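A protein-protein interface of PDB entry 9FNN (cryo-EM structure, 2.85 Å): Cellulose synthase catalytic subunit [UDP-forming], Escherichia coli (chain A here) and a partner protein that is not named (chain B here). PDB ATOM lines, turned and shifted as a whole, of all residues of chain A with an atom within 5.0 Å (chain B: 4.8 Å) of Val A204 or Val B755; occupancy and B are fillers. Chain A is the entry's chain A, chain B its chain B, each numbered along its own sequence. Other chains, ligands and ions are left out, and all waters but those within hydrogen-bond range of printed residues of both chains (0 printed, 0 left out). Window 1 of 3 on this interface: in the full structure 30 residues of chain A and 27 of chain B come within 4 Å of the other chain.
Of chain B, only Val B755 (3.95 Å) comes within 4 Å of Val A204. Of chain A, only Met A201 (3.5 Å), Val A204 (3.95 Å) and Leu A205 (3.8 Å) come within 4 Å of Val B755. Of the printed residues of chain A, Leu B762 touches Leu A200 (3.8 Å). Of the printed residues of chain B, Leu A205 touches Val B755. Printed residues of chain A within 4 Å of Ile B756: Met A201 (3.7 Å). Printed residues of chain A within 4 Å of Ala B759: Met A201. Of the printed residues of chain B, Leu A200 touches Leu B762 (3.8 Å). The nearest residue of chain A that does not touch Val B755 is Thr A208 (4.7 Å).
Leu A200 touches Leu B762 (CD1 to CB, 3.8 Å). O of Met A201 touches CG1 of Val B755, at 3.5 Å. Met A201 touches Ile B756 (CE to CG1, 3.7 Å). Met A201 touches Ala B759. Val A204 touches Val B755. Val B755 touches Leu A205 (CG2 to CD1, 3.8 Å).
Of the 9 printed residues of chain A, 4 touch a printed residue of chain B. Printed residues of chain A that touch a printed residue of chain B: Leu A200, Met A201, Val A204 and Leu A205. Hydrophobic or aromatic side chains of chain A that line the printed part of chain B: Leu A200, Met A201, Val A204 and Leu A205. Of the 10 printed residues of chain B, 4 touch a printed residue of chain A. Printed residues of chain B that touch a printed residue of chain A: Val B755, Ile B756, Ala B759 and Leu B762. Hydrophobic or aromatic side chains of chain B that line the printed part of chain A: Val B755, Ile B756, Ala B759 and Leu B762. Among the printed residues, 6 pairs touch across the chains. Among the printed residues, no Asp or Glu carboxylate lies within 4 Å of a Lys or Arg side-chain nitrogen of the other chain.
OG1 of Thr A208 lies close to O of Val A204 (3.3 Å). The backbone carbonyl oxygen (O) of Leu A205 sits at hydrogen-bond distance from the side-chain hydroxyl (OG1) of Thr A208.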
ATOM      1  N   LEU A 200      14.954 -14.648   6.603  1.00  0.00           N
ATOM      2  CA  LEU A 200      14.383 -15.390   7.723  1.00  0.00           C
ATOM      3  C   LEU A 200      12.905 -15.066   7.906  1.00  0.00           C
ATOM      4  O   LEU A 200      12.093 -15.962   8.171  1.00  0.00           O
ATOM      5  CB  LEU A 200      15.163 -15.087   9.002  1.00  0.00           C
ATOM      6  CG  LEU A 200      16.278 -16.061   9.379  1.00  0.00           C
ATOM      7  CD1 LEU A 200      15.706 -17.446   9.595  1.00  0.00           C
ATOM      8  CD2 LEU A 200      17.361 -16.089   8.323  1.00  0.00           C
ATOM      9  N   MET A 201      12.539 -13.790   7.774  1.00  0.00           N
ATOM     10  CA  MET A 201      11.138 -13.405   7.904  1.00  0.00           C
ATOM     11  C   MET A 201      10.281 -14.086   6.850  1.00  0.00           C
ATOM     12  O   MET A 201       9.192 -14.590   7.151  1.00  0.00           O
ATOM     13  CB  MET A 201      10.994 -11.888   7.796  1.00  0.00           C
ATOM     14  CG  MET A 201      11.562 -11.114   8.961  1.00  0.00           C
ATOM     15  SD  MET A 201      11.257  -9.348   8.805  1.00  0.00           S
ATOM     16  CE  MET A 201       9.471  -9.322   8.770  1.00  0.00           C
ATOM     17  N   LEU A 202      10.754 -14.106   5.605  1.00  0.00           N
ATOM     18  CA  LEU A 202      10.001 -14.762   4.546  1.00  0.00           C
ATOM     19  C   LEU A 202       9.892 -16.259   4.795  1.00  0.00           C
ATOM     20  O   LEU A 202       8.840 -16.858   4.544  1.00  0.00           O
ATOM     21  CB  LEU A 202      10.645 -14.485   3.191  1.00  0.00           C
ATOM     22  CG  LEU A 202      10.503 -13.055   2.675  1.00  0.00           C
ATOM     23  CD1 LEU A 202      10.842 -13.006   1.212  1.00  0.00           C
ATOM     24  CD2 LEU A 202       9.104 -12.529   2.909  1.00  0.00           C
ATOM     25  N   ILE A 203      10.962 -16.881   5.295  1.00  0.00           N
ATOM     26  CA  ILE A 203      10.914 -18.309   5.601  1.00  0.00           C
ATOM     27  C   ILE A 203       9.853 -18.592   6.655  1.00  0.00           C
ATOM     28  O   ILE A 203       9.054 -19.525   6.519  1.00  0.00           O
ATOM     29  CB  ILE A 203      12.297 -18.811   6.048  1.00  0.00           C
ATOM     30  CG1 ILE A 203      13.247 -18.894   4.857  1.00  0.00           C
ATOM     31  CG2 ILE A 203      12.182 -20.159   6.723  1.00  0.00           C
ATOM     32  CD1 ILE A 203      14.605 -19.425   5.209  1.00  0.00           C
ATOM     33  N   VAL A 204       9.818 -17.787   7.717  1.00  0.00           N
ATOM     34  CA  VAL A 204       8.859 -18.034   8.791  1.00  0.00           C
ATOM     35  C   VAL A 204       7.431 -17.789   8.312  1.00  0.00           C
ATOM     36  O   VAL A 204       6.514 -18.552   8.642  1.00  0.00           O
ATOM     37  CB  VAL A 204       9.200 -17.186  10.026  1.00  0.00           C
ATOM     38  CG1 VAL A 204       8.202 -17.440  11.130  1.00  0.00           C
ATOM     39  CG2 VAL A 204      10.593 -17.505  10.511  1.00  0.00           C
ATOM     40  N   LEU A 205       7.216 -16.726   7.532  1.00  0.00           N
ATOM     41  CA  LEU A 205       5.880 -16.457   7.005  1.00  0.00           C
ATOM     42  C   LEU A 205       5.411 -17.582   6.093  1.00  0.00           C
ATOM     43  O   LEU A 205       4.257 -18.033   6.179  1.00  0.00           O
ATOM     44  CB  LEU A 205       5.880 -15.124   6.261  1.00  0.00           C
ATOM     45  CG  LEU A 205       4.526 -14.549   5.870  1.00  0.00           C
ATOM     46  CD1 LEU A 205       3.693 -14.289   7.106  1.00  0.00           C
ATOM     47  CD2 LEU A 205       4.711 -13.278   5.073  1.00  0.00           C
ATOM     48  N   SER A 206       6.300 -18.063   5.222  1.00  0.00           N
ATOM     49  CA  SER A 206       5.962 -19.174   4.348  1.00  0.00           C
ATOM     50  C   SER A 206       5.661 -20.428   5.146  1.00  0.00           C
ATOM     51  O   SER A 206       4.761 -21.193   4.792  1.00  0.00           O
ATOM     52  CB  SER A 206       7.098 -19.429   3.364  1.00  0.00           C
ATOM     53  OG  SER A 206       6.884 -20.631   2.652  1.00  0.00           O
ATOM     54  N   LEU A 207       6.418 -20.669   6.214  1.00  0.00           N
ATOM     55  CA  LEU A 207       6.164 -21.850   7.028  1.00  0.00           C
ATOM     56  C   LEU A 207       4.807 -21.765   7.709  1.00  0.00           C
ATOM     57  O   LEU A 207       4.087 -22.765   7.783  1.00  0.00           O
ATOM     58  CB  LEU A 207       7.276 -22.040   8.054  1.00  0.00           C
ATOM     59  CG  LEU A 207       8.564 -22.668   7.527  1.00  0.00           C
ATOM     60  CD1 LEU A 207       9.474 -23.050   8.676  1.00  0.00           C
ATOM     61  CD2 LEU A 207       8.254 -23.871   6.667  1.00  0.00           C
ATOM     62  N   THR A 208       4.435 -20.584   8.202  1.00  0.00           N
ATOM     63  CA  THR A 208       3.109 -20.430   8.795  1.00  0.00           C
ATOM     64  C   THR A 208       2.012 -20.689   7.769  1.00  0.00           C
ATOM     65  O   THR A 208       1.045 -21.410   8.049  1.00  0.00           O
ATOM     66  CB  THR A 208       2.957 -19.037   9.402  1.00  0.00           C
ATOM     67  OG1 THR A 208       3.268 -18.046   8.415  1.00  0.00           O
ATOM     68  CG2 THR A 208       3.886 -18.873  10.587  1.00  0.00           C
ATOM     69  N   ALA B 751       0.180 -12.539  13.427  1.00  0.00           N
ATOM     70  CA  ALA B 751       1.082 -13.349  12.620  1.00  0.00           C
ATOM     71  C   ALA B 751       2.347 -12.580  12.266  1.00  0.00           C
ATOM     72  O   ALA B 751       3.447 -13.140  12.299  1.00  0.00           O
ATOM     73  CB  ALA B 751       0.370 -13.828  11.357  1.00  0.00           C
ATOM     74  N   ALA B 752       2.216 -11.296  11.928  1.00  0.00           N
ATOM     75  CA  ALA B 752       3.398 -10.492  11.633  1.00  0.00           C
ATOM     76  C   ALA B 752       4.285 -10.345  12.862  1.00  0.00           C
ATOM     77  O   ALA B 752       5.517 -10.410  12.760  1.00  0.00           O
ATOM     78  CB  ALA B 752       2.985  -9.123  11.098  1.00  0.00           C
ATOM     79  N   ILE B 753       3.678 -10.149  14.033  1.00  0.00           N
ATOM     80  CA  ILE B 753       4.453 -10.043  15.267  1.00  0.00           C
ATOM     81  C   ILE B 753       5.227 -11.332  15.516  1.00  0.00           C
ATOM     82  O   ILE B 753       6.427 -11.311  15.829  1.00  0.00           O
ATOM     83  CB  ILE B 753       3.529  -9.707  16.451  1.00  0.00           C
ATOM     84  CG1 ILE B 753       3.040  -8.260  16.352  1.00  0.00           C
ATOM     85  CG2 ILE B 753       4.235  -9.951  17.773  1.00  0.00           C
ATOM     86  CD1 ILE B 753       2.132  -7.845  17.488  1.00  0.00           C
ATOM     87  N   SER B 754       4.549 -12.471  15.376  1.00  0.00           N
ATOM     88  CA  SER B 754       5.205 -13.754  15.595  1.00  0.00           C
ATOM     89  C   SER B 754       6.328 -13.975  14.592  1.00  0.00           C
ATOM     90  O   SER B 754       7.404 -14.466  14.952  1.00  0.00           O
ATOM     91  CB  SER B 754       4.182 -14.885  15.516  1.00  0.00           C
ATOM     92  OG  SER B 754       3.551 -14.912  14.248  1.00  0.00           O
ATOM     93  N   VAL B 755       6.096 -13.611  13.331  1.00  0.00           N
ATOM     94  CA  VAL B 755       7.117 -13.778  12.303  1.00  0.00           C
ATOM     95  C   VAL B 755       8.348 -12.952  12.639  1.00  0.00           C
ATOM     96  O   VAL B 755       9.479 -13.446  12.575  1.00  0.00           O
ATOM     97  CB  VAL B 755       6.551 -13.413  10.921  1.00  0.00           C
ATOM     98  CG1 VAL B 755       7.674 -13.170   9.939  1.00  0.00           C
ATOM     99  CG2 VAL B 755       5.643 -14.514  10.417  1.00  0.00           C
ATOM    100  N   ILE B 756       8.151 -11.689  13.021  1.00  0.00           N
ATOM    101  CA  ILE B 756       9.289 -10.821  13.315  1.00  0.00           C
ATOM    102  C   ILE B 756      10.064 -11.334  14.522  1.00  0.00           C
ATOM    103  O   ILE B 756      11.302 -11.378  14.509  1.00  0.00           O
ATOM    104  CB  ILE B 756       8.822  -9.370  13.516  1.00  0.00           C
ATOM    105  CG1 ILE B 756       8.286  -8.801  12.205  1.00  0.00           C
ATOM    106  CG2 ILE B 756       9.960  -8.514  14.031  1.00  0.00           C
ATOM    107  CD1 ILE B 756       7.832  -7.367  12.304  1.00  0.00           C
ATOM    108  N   LEU B 757       9.360 -11.746  15.578  1.00  0.00           N
ATOM    109  CA  LEU B 757      10.058 -12.209  16.773  1.00  0.00           C
ATOM    110  C   LEU B 757      10.817 -13.512  16.523  1.00  0.00           C
ATOM    111  O   LEU B 757      11.975 -13.654  16.947  1.00  0.00           O
ATOM    112  CB  LEU B 757       9.069 -12.365  17.925  1.00  0.00           C
ATOM    113  CG  LEU B 757       8.609 -11.044  18.540  1.00  0.00           C
ATOM    114  CD1 LEU B 757       7.538 -11.281  19.585  1.00  0.00           C
ATOM    115  CD2 LEU B 757       9.787 -10.313  19.148  1.00  0.00           C
ATOM    116  N   LEU B 758      10.192 -14.477  15.842  1.00  0.00           N
ATOM    117  CA  LEU B 758      10.890 -15.722  15.536  1.00  0.00           C
ATOM    118  C   LEU B 758      12.059 -15.478  14.597  1.00  0.00           C
ATOM    119  O   LEU B 758      13.107 -16.121  14.723  1.00  0.00           O
ATOM    120  CB  LEU B 758       9.926 -16.739  14.936  1.00  0.00           C
ATOM    121  CG  LEU B 758       9.071 -17.510  15.934  1.00  0.00           C
ATOM    122  CD1 LEU B 758       8.143 -18.464  15.212  1.00  0.00           C
ATOM    123  CD2 LEU B 758       9.954 -18.256  16.910  1.00  0.00           C
ATOM    124  N   ALA B 759      11.903 -14.550  13.651  1.00  0.00           N
ATOM    125  CA  ALA B 759      13.013 -14.195  12.781  1.00  0.00           C
ATOM    126  C   ALA B 759      14.167 -13.611  13.579  1.00  0.00           C
ATOM    127  O   ALA B 759      15.329 -13.918  13.307  1.00  0.00           O
ATOM    128  CB  ALA B 759      12.545 -13.212  11.711  1.00  0.00           C
ATOM    129  N   LEU B 762      15.879 -16.555  15.509  1.00  0.00           N
ATOM    130  CA  LEU B 762      16.651 -17.374  14.586  1.00  0.00           C
ATOM    131  C   LEU B 762      17.874 -16.627  14.078  1.00  0.00           C
ATOM    132  O   LEU B 762      18.941 -17.222  13.908  1.00  0.00           O
ATOM    133  CB  LEU B 762      15.775 -17.819  13.418  1.00  0.00           C
ATOM    134  CG  LEU B 762      14.704 -18.855  13.747  1.00  0.00           C
ATOM    135  CD1 LEU B 762      13.910 -19.208  12.502  1.00  0.00           C
ATOM    136  CD2 LEU B 762      15.334 -20.093  14.354  1.00  0.00           C
